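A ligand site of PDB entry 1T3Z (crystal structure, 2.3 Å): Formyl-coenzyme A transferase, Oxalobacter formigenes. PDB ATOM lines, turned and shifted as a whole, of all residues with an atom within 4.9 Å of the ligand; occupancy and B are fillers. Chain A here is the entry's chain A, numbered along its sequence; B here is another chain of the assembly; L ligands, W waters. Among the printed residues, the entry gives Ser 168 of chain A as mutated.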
ATOM      1  N   HIS A  14       0.591  13.656  22.251  1.00  0.00           N
ATOM      2  CA  HIS A  14       0.007  13.944  23.560  1.00  0.00           C
ATOM      3  C   HIS A  14       0.823  15.031  24.327  1.00  0.00           C
ATOM      4  O   HIS A  14       1.907  15.397  23.912  1.00  0.00           O
ATOM      5  CB  HIS A  14      -0.104  12.647  24.371  1.00  0.00           C
ATOM      6  CG  HIS A  14       1.198  11.976  24.644  1.00  0.00           C
ATOM      7  ND1 HIS A  14       1.316  10.888  25.478  1.00  0.00           N
ATOM      8  CD2 HIS A  14       2.464  12.253  24.225  1.00  0.00           C
ATOM      9  CE1 HIS A  14       2.578  10.520  25.552  1.00  0.00           C
ATOM     10  NE2 HIS A  14       3.302  11.327  24.808  1.00  0.00           N
ATOM     11  N   VAL A  15       0.289  15.518  25.434  1.00  0.00           N
ATOM     12  CA  VAL A  15       0.947  16.539  26.268  1.00  0.00           C
ATOM     13  C   VAL A  15       1.063  17.875  25.527  1.00  0.00           C
ATOM     14  O   VAL A  15       0.039  18.445  25.148  1.00  0.00           O
ATOM     15  CB  VAL A  15       2.316  16.070  26.878  1.00  0.00           C
ATOM     16  CG1 VAL A  15       2.673  16.939  28.089  1.00  0.00           C
ATOM     17  CG2 VAL A  15       2.289  14.594  27.314  1.00  0.00           C
ATOM     18  N   GLN A  16       2.278  18.379  25.270  1.00  0.00           N
ATOM     19  CA  GLN A  16       2.406  19.782  24.828  1.00  0.00           C
ATOM     20  C   GLN A  16       3.110  19.990  23.510  1.00  0.00           C
ATOM     21  O   GLN A  16       2.552  20.622  22.605  1.00  0.00           O
ATOM     22  CB  GLN A  16       3.018  20.698  25.920  1.00  0.00           C
ATOM     23  CG  GLN A  16       3.170  22.160  25.423  1.00  0.00           C
ATOM     24  CD  GLN A  16       3.442  23.234  26.488  1.00  0.00           C
ATOM     25  OE1 GLN A  16       3.473  22.960  27.703  1.00  0.00           O
ATOM     26  NE2 GLN A  16       3.621  24.484  26.007  1.00  0.00           N
ATOM     27  N   ALA A  17       4.323  19.463  23.379  1.00  0.00           N
ATOM     28  CA  ALA A  17       5.118  19.736  22.192  1.00  0.00           C
ATOM     29  C   ALA A  17       4.402  19.314  20.903  1.00  0.00           C
ATOM     30  O   ALA A  17       4.185  20.136  20.006  1.00  0.00           O
ATOM     31  CB  ALA A  17       6.469  19.088  22.309  1.00  0.00           C
ATOM     32  N   GLY A  18       4.014  18.050  20.820  1.00  0.00           N
ATOM     33  CA  GLY A  18       3.378  17.526  19.629  1.00  0.00           C
ATOM     34  C   GLY A  18       2.037  18.187  19.347  1.00  0.00           C
ATOM     35  O   GLY A  18       1.794  18.640  18.214  1.00  0.00           O
ATOM     36  N   GLU A  36      -6.073   8.869  20.165  1.00  0.00           N
ATOM     37  CA  GLU A  36      -5.961   8.884  21.615  1.00  0.00           C
ATOM     38  C   GLU A  36      -6.167   7.497  22.232  1.00  0.00           C
ATOM     39  O   GLU A  36      -6.765   6.611  21.615  1.00  0.00           O
ATOM     40  CB  GLU A  36      -6.997   9.849  22.195  1.00  0.00           C
ATOM     41  CG  GLU A  36      -6.856  11.285  21.688  1.00  0.00           C
ATOM     42  CD  GLU A  36      -7.727  12.246  22.456  1.00  0.00           C
ATOM     43  OE1 GLU A  36      -7.480  12.381  23.673  1.00  0.00           O
ATOM     44  OE2 GLU A  36      -8.649  12.857  21.850  1.00  0.00           O
ATOM     45  N   ARG A  37      -5.688   7.309  23.464  1.00  0.00           N
ATOM     46  CA  ARG A  37      -5.874   6.066  24.211  1.00  0.00           C
ATOM     47  C   ARG A  37      -7.357   5.896  24.543  1.00  0.00           C
ATOM     48  O   ARG A  37      -8.011   6.828  25.008  1.00  0.00           O
ATOM     49  CB  ARG A  37      -5.085   6.051  25.546  1.00  0.00           C
ATOM     50  CG  ARG A  37      -3.559   6.292  25.482  1.00  0.00           C
ATOM     51  CD  ARG A  37      -2.935   6.586  26.860  1.00  0.00           C
ATOM     52  NE  ARG A  37      -1.496   6.885  26.833  1.00  0.00           N
ATOM     53  CZ  ARG A  37      -0.498   5.990  26.988  1.00  0.00           C
ATOM     54  NH1 ARG A  37      -0.746   4.688  27.166  1.00  0.00           N
ATOM     55  NH2 ARG A  37       0.770   6.409  26.962  1.00  0.00           N
ATOM     56  N   ARG A  38      -7.841   4.682  24.325  1.00  0.00           N
ATOM     57  CA  ARG A  38      -9.225   4.309  24.602  1.00  0.00           C
ATOM     58  C   ARG A  38      -9.482   4.383  26.115  1.00  0.00           C
ATOM     59  O   ARG A  38      -8.823   3.678  26.882  1.00  0.00           O
ATOM     60  CB  ARG A  38      -9.461   2.889  24.072  1.00  0.00           C
ATOM     61  CG  ARG A  38     -10.889   2.572  23.666  1.00  0.00           C
ATOM     62  CD  ARG A  38     -11.140   1.079  23.476  1.00  0.00           C
ATOM     63  NE  ARG A  38     -11.041   0.384  24.758  1.00  0.00           N
ATOM     64  CZ  ARG A  38     -12.071   0.097  25.552  1.00  0.00           C
ATOM     65  NH1 ARG A  38     -13.320   0.408  25.221  1.00  0.00           N
ATOM     66  NH2 ARG A  38     -11.835  -0.525  26.697  1.00  0.00           N
ATOM     67  N   TYR A  58      -5.905  22.848  29.937  1.00  0.00           N
ATOM     68  CA  TYR A  58      -4.674  22.307  29.344  1.00  0.00           C
ATOM     69  C   TYR A  58      -4.961  21.589  28.040  1.00  0.00           C
ATOM     70  O   TYR A  58      -4.297  21.830  27.024  1.00  0.00           O
ATOM     71  CB  TYR A  58      -3.946  21.355  30.301  1.00  0.00           C
ATOM     72  CG  TYR A  58      -2.470  21.099  30.024  1.00  0.00           C
ATOM     73  CD1 TYR A  58      -1.667  20.474  30.994  1.00  0.00           C
ATOM     74  CD2 TYR A  58      -1.861  21.475  28.839  1.00  0.00           C
ATOM     75  CE1 TYR A  58      -0.305  20.239  30.757  1.00  0.00           C
ATOM     76  CE2 TYR A  58      -0.540  21.239  28.604  1.00  0.00           C
ATOM     77  CZ  TYR A  58       0.238  20.626  29.550  1.00  0.00           C
ATOM     78  OH  TYR A  58       1.563  20.407  29.260  1.00  0.00           O
ATOM     79  N   LEU A  71      -8.444   4.748  19.823  1.00  0.00           N
ATOM     80  CA  LEU A  71      -7.907   3.579  19.131  1.00  0.00           C
ATOM     81  C   LEU A  71      -6.876   2.864  20.011  1.00  0.00           C
ATOM     82  O   LEU A  71      -5.913   3.478  20.442  1.00  0.00           O
ATOM     83  CB  LEU A  71      -7.289   3.997  17.786  1.00  0.00           C
ATOM     84  CG  LEU A  71      -6.662   2.939  16.867  1.00  0.00           C
ATOM     85  CD1 LEU A  71      -7.599   1.749  16.702  1.00  0.00           C
ATOM     86  CD2 LEU A  71      -6.326   3.500  15.500  1.00  0.00           C
ATOM     87  N   ASP A  72      -7.114   1.595  20.317  1.00  0.00           N
ATOM     88  CA  ASP A  72      -6.120   0.728  20.971  1.00  0.00           C
ATOM     89  C   ASP A  72      -5.196   0.172  19.873  1.00  0.00           C
ATOM     90  O   ASP A  72      -5.603  -0.683  19.073  1.00  0.00           O
ATOM     91  CB  ASP A  72      -6.804  -0.407  21.764  1.00  0.00           C
ATOM     92  CG  ASP A  72      -5.819  -1.288  22.558  1.00  0.00           C
ATOM     93  OD1 ASP A  72      -4.723  -1.578  22.066  1.00  0.00           O
ATOM     94  OD2 ASP A  72      -6.070  -1.761  23.696  1.00  0.00           O
ATOM     95  N   MET A  73      -3.952   0.666  19.842  1.00  0.00           N
ATOM     96  CA  MET A  73      -2.956   0.291  18.833  1.00  0.00           C
ATOM     97  C   MET A  73      -2.185  -1.002  19.170  1.00  0.00           C
ATOM     98  O   MET A  73      -1.471  -1.542  18.315  1.00  0.00           O
ATOM     99  CB  MET A  73      -1.955   1.436  18.612  1.00  0.00           C
ATOM    100  CG  MET A  73      -2.335   2.424  17.519  1.00  0.00           C
ATOM    101  SD  MET A  73      -2.340   4.176  18.060  1.00  0.00           S
ATOM    102  CE  MET A  73      -0.826   4.357  18.881  1.00  0.00           C
ATOM    103  N   LYS A  74      -2.304  -1.476  20.407  1.00  0.00           N
ATOM    104  CA  LYS A  74      -1.741  -2.756  20.831  1.00  0.00           C
ATOM    105  C   LYS A  74      -2.556  -3.978  20.336  1.00  0.00           C
ATOM    106  O   LYS A  74      -2.093  -5.116  20.496  1.00  0.00           O
ATOM    107  CB  LYS A  74      -1.582  -2.809  22.365  1.00  0.00           C
ATOM    108  CG  LYS A  74      -0.482  -1.899  22.923  1.00  0.00           C
ATOM    109  CD  LYS A  74      -0.716  -1.566  24.415  1.00  0.00           C
ATOM    110  CE  LYS A  74       0.572  -1.071  25.123  1.00  0.00           C
ATOM    111  NZ  LYS A  74       0.378   0.180  25.945  1.00  0.00           N
ATOM    112  N   ASN A  95       4.917  12.245  19.268  1.00  0.00           N
ATOM    113  CA  ASN A  95       5.846  12.584  20.354  1.00  0.00           C
ATOM    114  C   ASN A  95       5.690  11.615  21.503  1.00  0.00           C
ATOM    115  O   ASN A  95       5.474  12.035  22.639  1.00  0.00           O
ATOM    116  CB  ASN A  95       5.727  14.059  20.821  1.00  0.00           C
ATOM    117  CG  ASN A  95       4.440  14.352  21.596  1.00  0.00           C
ATOM    118  OD1 ASN A  95       3.370  13.848  21.249  1.00  0.00           O
ATOM    119  ND2 ASN A  95       4.537  15.193  22.648  1.00  0.00           N
ATOM    120  N   PHE A  96       5.764  10.327  21.158  1.00  0.00           N
ATOM    121  CA  PHE A  96       5.846   9.222  22.103  1.00  0.00           C
ATOM    122  C   PHE A  96       7.302   9.076  22.493  1.00  0.00           C
ATOM    123  O   PHE A  96       8.183   9.678  21.875  1.00  0.00           O
ATOM    124  CB  PHE A  96       5.420   7.870  21.467  1.00  0.00           C
ATOM    125  CG  PHE A  96       3.922   7.689  21.248  1.00  0.00           C
ATOM    126  CD1 PHE A  96       3.456   7.069  20.074  1.00  0.00           C
ATOM    127  CD2 PHE A  96       2.990   8.103  22.207  1.00  0.00           C
ATOM    128  CE1 PHE A  96       2.097   6.878  19.857  1.00  0.00           C
ATOM    129  CE2 PHE A  96       1.618   7.915  21.985  1.00  0.00           C
ATOM    130  CZ  PHE A  96       1.172   7.291  20.800  1.00  0.00           C
ATOM    131  N   GLY A  97       7.555   8.191  23.468  1.00  0.00           N
ATOM    132  CA  GLY A  97       8.917   7.864  23.878  1.00  0.00           C
ATOM    133  C   GLY A  97       9.782   7.419  22.716  1.00  0.00           C
ATOM    134  O   GLY A  97       9.273   6.925  21.715  1.00  0.00           O
ATOM    135  N   PRO A  98      11.095   7.591  22.858  1.00  0.00           N
ATOM    136  CA  PRO A  98      12.103   7.323  21.802  1.00  0.00           C
ATOM    137  C   PRO A  98      11.863   6.247  20.719  1.00  0.00           C
ATOM    138  O   PRO A  98      12.084   6.560  19.522  1.00  0.00           O
ATOM    139  CB  PRO A  98      13.344   7.009  22.618  1.00  0.00           C
ATOM    140  CG  PRO A  98      13.232   7.959  23.768  1.00  0.00           C
ATOM    141  CD  PRO A  98      11.746   8.100  24.080  1.00  0.00           C
ATOM    142  N   ALA A 100       8.874   4.075  20.531  1.00  0.00           N
ATOM    143  CA  ALA A 100       7.536   3.516  20.755  1.00  0.00           C
ATOM    144  C   ALA A 100       6.782   3.180  19.467  1.00  0.00           C
ATOM    145  O   ALA A 100       6.234   2.093  19.339  1.00  0.00           O
ATOM    146  CB  ALA A 100       6.719   4.458  21.628  1.00  0.00           C
ATOM    147  N   ARG A 103       8.338  -0.022  17.921  1.00  0.00           N
ATOM    148  CA  ARG A 103       7.836  -1.168  18.690  1.00  0.00           C
ATOM    149  C   ARG A 103       6.417  -1.593  18.283  1.00  0.00           C
ATOM    150  O   ARG A 103       6.072  -2.750  18.398  1.00  0.00           O
ATOM    151  CB  ARG A 103       7.808  -0.830  20.188  1.00  0.00           C
ATOM    152  CG  ARG A 103       9.115  -0.966  20.953  1.00  0.00           C
ATOM    153  CD  ARG A 103       8.933  -0.707  22.457  1.00  0.00           C
ATOM    154  NE  ARG A 103      10.017   0.087  23.067  1.00  0.00           N
ATOM    155  CZ  ARG A 103       9.922   1.340  23.529  1.00  0.00           C
ATOM    156  NH1 ARG A 103       8.791   2.027  23.485  1.00  0.00           N
ATOM    157  NH2 ARG A 103      10.986   1.910  24.066  1.00  0.00           N
ATOM    158  N   MET A 104       5.611  -0.629  17.838  1.00  0.00           N
ATOM    159  CA  MET A 104       4.240  -0.859  17.435  1.00  0.00           C
ATOM    160  C   MET A 104       4.116  -1.477  16.041  1.00  0.00           C
ATOM    161  O   MET A 104       3.009  -1.733  15.580  1.00  0.00           O
ATOM    162  CB  MET A 104       3.459   0.459  17.457  1.00  0.00           C
ATOM    163  CG  MET A 104       2.500   0.603  18.610  1.00  0.00           C
ATOM    164  SD  MET A 104       2.167   2.348  18.945  1.00  0.00           S
ATOM    165  CE  MET A 104       1.168   2.175  20.457  1.00  0.00           C
ATOM    166  N   VAL A 123       8.846  14.630  17.718  1.00  0.00           N
ATOM    167  CA  VAL A 123       9.562  15.289  18.778  1.00  0.00           C
ATOM    168  C   VAL A 123      10.182  14.253  19.666  1.00  0.00           C
ATOM    169  O   VAL A 123       9.532  13.304  20.043  1.00  0.00           O
ATOM    170  CB  VAL A 123       8.649  16.136  19.661  1.00  0.00           C
ATOM    171  CG1 VAL A 123       9.502  16.897  20.695  1.00  0.00           C
ATOM    172  CG2 VAL A 123       7.832  17.094  18.805  1.00  0.00           C
ATOM    173  N   LYS A 124      11.441  14.466  20.022  1.00  0.00           N
ATOM    174  CA  LYS A 124      12.148  13.644  21.005  1.00  0.00           C
ATOM    175  C   LYS A 124      12.876  14.539  21.996  1.00  0.00           C
ATOM    176  O   LYS A 124      13.019  15.721  21.758  1.00  0.00           O
ATOM    177  CB  LYS A 124      13.153  12.734  20.274  1.00  0.00           C
ATOM    178  CG  LYS A 124      12.484  11.678  19.349  1.00  0.00           C
ATOM    179  CD  LYS A 124      11.747  10.569  20.156  1.00  0.00           C
ATOM    180  CE  LYS A 124      10.744   9.729  19.305  1.00  0.00           C
ATOM    181  NZ  LYS A 124       9.308  10.226  19.374  1.00  0.00           N
ATOM    182  N   GLY A 125      13.303  13.967  23.120  1.00  0.00           N
ATOM    183  CA  GLY A 125      14.102  14.693  24.088  1.00  0.00           C
ATOM    184  C   GLY A 125      15.461  15.102  23.543  1.00  0.00           C
ATOM    185  O   GLY A 125      15.876  16.245  23.664  1.00  0.00           O
ATOM    186  N   LEU A 135      16.235   8.860  26.362  1.00  0.00           N
ATOM    187  CA  LEU A 135      15.652   9.436  27.571  1.00  0.00           C
ATOM    188  C   LEU A 135      14.322  10.123  27.299  1.00  0.00           C
ATOM    189  O   LEU A 135      14.188  10.884  26.333  1.00  0.00           O
ATOM    190  CB  LEU A 135      16.596  10.431  28.238  1.00  0.00           C
ATOM    191  CG  LEU A 135      17.946   9.878  28.666  1.00  0.00           C
ATOM    192  CD1 LEU A 135      18.676  10.922  29.498  1.00  0.00           C
ATOM    193  CD2 LEU A 135      17.800   8.543  29.425  1.00  0.00           C
ATOM    194  N   LYS A 136      13.363   9.847  28.179  1.00  0.00           N
ATOM    195  CA  LYS A 136      12.103  10.577  28.261  1.00  0.00           C
ATOM    196  C   LYS A 136      12.371  11.939  28.919  1.00  0.00           C
ATOM    197  O   LYS A 136      13.077  12.033  29.928  1.00  0.00           O
ATOM    198  CB  LYS A 136      11.072   9.772  29.071  1.00  0.00           C
ATOM    199  CG  LYS A 136      10.713   8.409  28.457  1.00  0.00           C
ATOM    200  CD  LYS A 136       9.528   7.741  29.181  1.00  0.00           C
ATOM    201  CE  LYS A 136       9.333   6.288  28.719  1.00  0.00           C
ATOM    202  NZ  LYS A 136       8.399   5.509  29.619  1.00  0.00           N
ATOM    203  N   VAL A 137      11.849  12.988  28.315  1.00  0.00           N
ATOM    204  CA  VAL A 137      12.015  14.321  28.874  1.00  0.00           C
ATOM    205  C   VAL A 137      10.722  15.105  28.734  1.00  0.00           C
ATOM    206  O   VAL A 137       9.965  14.917  27.781  1.00  0.00           O
ATOM    207  CB  VAL A 137      13.272  15.105  28.304  1.00  0.00           C
ATOM    208  CG1 VAL A 137      14.157  14.225  27.446  1.00  0.00           C
ATOM    209  CG2 VAL A 137      12.906  16.417  27.574  1.00  0.00           C
ATOM    210  N   TYR A 138      10.484  15.935  29.740  1.00  0.00           N
ATOM    211  CA  TYR A 138       9.430  16.931  29.748  1.00  0.00           C
ATOM    212  C   TYR A 138      10.043  18.339  29.741  1.00  0.00           C
ATOM    213  O   TYR A 138      11.249  18.503  29.963  1.00  0.00           O
ATOM    214  CB  TYR A 138       8.601  16.785  31.030  1.00  0.00           C
ATOM    215  CG  TYR A 138       7.627  15.638  31.056  1.00  0.00           C
ATOM    216  CD1 TYR A 138       6.295  15.836  30.673  1.00  0.00           C
ATOM    217  CD2 TYR A 138       8.013  14.371  31.511  1.00  0.00           C
ATOM    218  CE1 TYR A 138       5.379  14.792  30.709  1.00  0.00           C
ATOM    219  CE2 TYR A 138       7.096  13.306  31.553  1.00  0.00           C
ATOM    220  CZ  TYR A 138       5.781  13.534  31.152  1.00  0.00           C
ATOM    221  OH  TYR A 138       4.855  12.531  31.183  1.00  0.00           O
ATOM    222  N   GLU A 139       9.189  19.336  29.544  1.00  0.00           N
ATOM    223  CA  GLU A 139       9.502  20.763  29.486  1.00  0.00           C
ATOM    224  C   GLU A 139      10.808  21.212  30.195  1.00  0.00           C
ATOM    225  O   GLU A 139      11.741  21.625  29.547  1.00  0.00           O
ATOM    226  CB  GLU A 139       8.293  21.544  30.027  1.00  0.00           C
ATOM    227  CG  GLU A 139       8.449  23.059  30.101  1.00  0.00           C
ATOM    228  CD  GLU A 139       8.881  23.701  28.786  1.00  0.00           C
ATOM    229  OE1 GLU A 139       9.922  24.395  28.754  1.00  0.00           O
ATOM    230  OE2 GLU A 139       8.188  23.506  27.772  1.00  0.00           O
ATOM    231  N   SER A 168       9.040  22.540  25.136  1.00  0.00           N
ATOM    232  CA  SER A 168       7.932  21.771  24.546  1.00  0.00           C
ATOM    233  C   SER A 168       7.170  22.545  23.453  1.00  0.00           C
ATOM    234  O   SER A 168       7.279  22.201  22.302  1.00  0.00           O
ATOM    235  CB  SER A 168       7.006  21.289  25.650  1.00  0.00           C
ATOM    236  OG  SER A 168       6.294  22.372  26.207  1.00  0.00           O
ATOM    237  N   MET A 199      14.169  18.244  21.699  1.00  0.00           N
ATOM    238  CA  MET A 199      13.842  19.319  22.600  1.00  0.00           C
ATOM    239  C   MET A 199      15.086  20.044  23.047  1.00  0.00           C
ATOM    240  O   MET A 199      15.064  21.274  23.171  1.00  0.00           O
ATOM    241  CB  MET A 199      13.099  18.775  23.813  1.00  0.00           C
ATOM    242  CG  MET A 199      11.651  18.330  23.476  1.00  0.00           C
ATOM    243  SD  MET A 199      10.928  17.314  24.801  1.00  0.00           S
ATOM    244  CE  MET A 199      10.356  18.558  25.758  1.00  0.00           C
ATOM    245  N   ASN B 286       2.243   8.818  36.833  1.00  0.00           N
ATOM    246  CA  ASN B 286       2.271   7.419  36.389  1.00  0.00           C
ATOM    247  C   ASN B 286       3.563   6.657  36.715  1.00  0.00           C
ATOM    248  O   ASN B 286       3.588   5.423  36.674  1.00  0.00           O
ATOM    249  CB  ASN B 286       1.968   7.324  34.885  1.00  0.00           C
ATOM    250  CG  ASN B 286       3.120   7.807  34.014  1.00  0.00           C
ATOM    251  OD1 ASN B 286       3.830   8.747  34.369  1.00  0.00           O
ATOM    252  ND2 ASN B 286       3.289   7.163  32.869  1.00  0.00           N
ATOM    253  N   MET B 287       4.630   7.377  37.031  1.00  0.00           N
ATOM    254  CA  MET B 287       5.907   6.765  37.424  1.00  0.00           C
ATOM    255  C   MET B 287       6.188   6.905  38.917  1.00  0.00           C
ATOM    256  O   MET B 287       7.350   6.868  39.325  1.00  0.00           O
ATOM    257  CB  MET B 287       7.053   7.405  36.659  1.00  0.00           C
ATOM    258  CG  MET B 287       7.047   7.155  35.171  1.00  0.00           C
ATOM    259  SD  MET B 287       8.345   8.102  34.414  1.00  0.00           S
ATOM    260  CE  MET B 287       7.423   8.988  33.101  1.00  0.00           C
HETATM  261  N1  LIG L   1      -2.722   2.657  22.495  1.00  0.00           N
HETATM  262  C1  LIG L   1      -1.741   1.801  22.830  1.00  0.00           C
HETATM  263  N2  LIG L   1      -0.534   2.215  23.261  1.00  0.00           N
HETATM  264  C2  LIG L   1      -0.262   3.541  23.363  1.00  0.00           C
HETATM  265  C3  LIG L   1      -1.255   4.519  23.027  1.00  0.00           C
HETATM  266  C4  LIG L   1      -2.567   4.003  22.566  1.00  0.00           C
HETATM  267  N3  LIG L   1      -3.557   4.849  22.227  1.00  0.00           N
HETATM  268  N4  LIG L   1      -0.716   5.774  23.236  1.00  0.00           N
HETATM  269  C5  LIG L   1       0.580   5.495  23.686  1.00  0.00           C
HETATM  270  N5  LIG L   1       0.838   4.155  23.770  1.00  0.00           N
HETATM  271  C6  LIG L   1       2.025   3.325  24.166  1.00  0.00           C
HETATM  272  C7  LIG L   1       3.307   3.622  23.384  1.00  0.00           C
HETATM  273  O1  LIG L   1       3.562   2.735  22.299  1.00  0.00           O
HETATM  274  C8  LIG L   1       4.412   3.632  24.425  1.00  0.00           C
HETATM  275  O2  LIG L   1       5.290   2.539  24.070  1.00  0.00           O
HETATM  276  P1  LIG L   1       5.921   1.377  24.996  1.00  0.00           P
HETATM  277  O3  LIG L   1       6.416   0.204  24.043  1.00  0.00           O
HETATM  278  O4  LIG L   1       4.856   0.755  25.995  1.00  0.00           O
HETATM  279  O5  LIG L   1       7.153   1.962  25.823  1.00  0.00           O
HETATM  280  C9  LIG L   1       3.744   3.491  25.801  1.00  0.00           C
HETATM  281  O6  LIG L   1       2.335   3.359  25.574  1.00  0.00           O
HETATM  282  C10 LIG L   1       4.102   4.618  26.776  1.00  0.00           C
HETATM  283  O7  LIG L   1       4.108   5.879  26.109  1.00  0.00           O
HETATM  284  P2  LIG L   1       5.031   7.122  26.568  1.00  0.00           P
HETATM  285  O8  LIG L   1       4.994   8.205  25.410  1.00  0.00           O
HETATM  286  O9  LIG L   1       6.515   6.693  26.918  1.00  0.00           O
HETATM  287  O10 LIG L   1       4.275   7.605  27.894  1.00  0.00           O
HETATM  288  P3  LIG L   1       5.102   8.302  29.056  1.00  0.00           P
HETATM  289  O11 LIG L   1       6.324   7.410  29.530  1.00  0.00           O
HETATM  290  O12 LIG L   1       4.182   8.692  30.290  1.00  0.00           O
HETATM  291  O13 LIG L   1       5.561   9.631  28.253  1.00  0.00           O
HETATM  292  C11 LIG L   1       6.960  11.578  27.714  1.00  0.00           C
HETATM  293  C12 LIG L   1       6.468  10.586  28.773  1.00  0.00           C
HETATM  294  C13 LIG L   1       5.903  12.646  27.405  1.00  0.00           C
HETATM  295  C14 LIG L   1       8.156  12.275  28.329  1.00  0.00           C
HETATM  296  C15 LIG L   1       7.278  10.813  26.415  1.00  0.00           C
HETATM  297  O14 LIG L   1       6.086  10.618  25.654  1.00  0.00           O
HETATM  298  C16 LIG L   1       8.327  11.523  25.571  1.00  0.00           C
HETATM  299  O15 LIG L   1       9.499  11.392  25.854  1.00  0.00           O
HETATM  300  N6  LIG L   1       7.897  12.283  24.568  1.00  0.00           N
HETATM  301  C17 LIG L   1       8.778  13.118  23.757  1.00  0.00           C
HETATM  302  C18 LIG L   1       8.935  14.461  24.475  1.00  0.00           C
HETATM  303  C19 LIG L   1       7.710  15.360  24.312  1.00  0.00           C
HETATM  304  O16 LIG L   1       7.285  15.529  23.184  1.00  0.00           O
HETATM  305  N7  LIG L   1       7.185  15.987  25.401  1.00  0.00           N
HETATM  306  C20 LIG L   1       6.157  17.061  25.217  1.00  0.00           C
HETATM  307  C21 LIG L   1       5.442  17.642  26.421  1.00  0.00           C
HETATM  308  S1  LIG L   1       6.534  18.153  27.710  1.00  0.00           S
HETATM  309  O17 LIG L   1       5.943  19.166  28.739  1.00  0.00           O
HETATM  310  O   HOH W   1      11.971  11.913  25.036  1.00  0.00           O
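Water W1 lies within hydrogen-bond range of O15 of the ligand (2.7 Å), O of Leu 135 (2.8 Å), N of Gly 125 (3.1 Å) and N of Val 137 (3.5 Å).
The side-chain carboxylate of Glu 139 is in hydrogen-bond range of the side-chain hydroxyl of Ser 168. ND2 of Asn 95 lies close to N of Gly 18 (3.4 Å). OG of Ser 168 lies close to OE1 of Gln 16, 3.2 Å away. The side-chain amino group of Lys 124 is in hydrogen-bond range of the backbone carbonyl oxygen of Phe 96 (2.8 Å). The backbone carbonyl oxygen of Gly 125 is in hydrogen-bond range of the backbone NH of Met 199, at 3.3 Å. N of Leu 71 sits at hydrogen-bond distance from O of Glu 36 (3.1 Å). The backbone NH of Met 199 is in hydrogen-bond range of the backbone carbonyl oxygen of Lys 124 (2.8 Å). The backbone NH of Lys 74 is in hydrogen-bond range of the side-chain carboxylate of Asp 72 (2.9 Å).
NE2 of His 14 lies within hydrogen-bond range of O14 of the ligand. An oxygen (O11) of the ligand lies within salt-bridge range of the side-chain amino group (NZ) of Lys 136. The backbone carbonyl oxygen (O) of Asn 95 sits at hydrogen-bond distance from a nitrogen (N6) of the ligand (3.1 Å). The guanidinium group (NH2) of Arg 37 lies close to an oxygen (O7) of the ligand (3.5 Å). The side-chain amino group (NZ) of Lys 74 lies within hydrogen-bond range of a nitrogen (N2) of the ligand (3.5 Å). The side-chain amide nitrogen of Asn 286 of chain B sits at hydrogen-bond distance from an oxygen (O12) of the ligand, 3.1 Å away. An oxygen (O8) of the ligand sits at hydrogen-bond distance from the backbone NH (N) of Gly 97 (3.2 Å). An oxygen (O16) of the ligand lies within hydrogen-bond range of the side-chain amide nitrogen of Asn 95 (2.8 Å). The guanidinium group (NH1) of Arg 103 is in salt-bridge range of an oxygen (O5) of the ligand. O of Leu 71 lies within hydrogen-bond range of N3 of the ligand (3.3 Å). SD of Met 104 sits close to O1 of the ligand, at 3.7 Å. N of Glu 139 is in hydrogen-bond range of O17 of the ligand, at 3.3 Å.
CG1 of Val 15 touches C21 of the ligand (3.3 Å). N of Gln 16 touches C21 of the ligand (3.4 Å). N of Ala 17 touches C20 of the ligand, 3.5 Å away. Glu 36 touches the ligand (O to N3, 3.7 Å). N of Met 73 touches N1 of the ligand, at 3.5 Å. Phe 96 touches the ligand (CE2 to C5, 3.1 Å). Ala 100 touches the ligand (CB to O2, 3.4 Å). CG1 of Val 123 touches O16 of the ligand, 3.6 Å away. O of Val 137 touches C14 of the ligand, 3.2 Å away. Tyr 138 touches the ligand. Ser 168 touches the ligand (CB to S1, 3.8 Å). SD of Met 199 touches C18 of the ligand (3.5 Å). Hydrophobic or aromatic side chains within 4 Å of the ligand: His 14, Val 15, Ala 17, Phe 96, Ala 100, Met 104, Val 123, Tyr 138 and Met 199. Along chain A the residues within 4 Å of the ligand span positions 14 to 199. The nearest printed residue that does not touch the ligand is Met 287 of chain B (4.1 Å).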
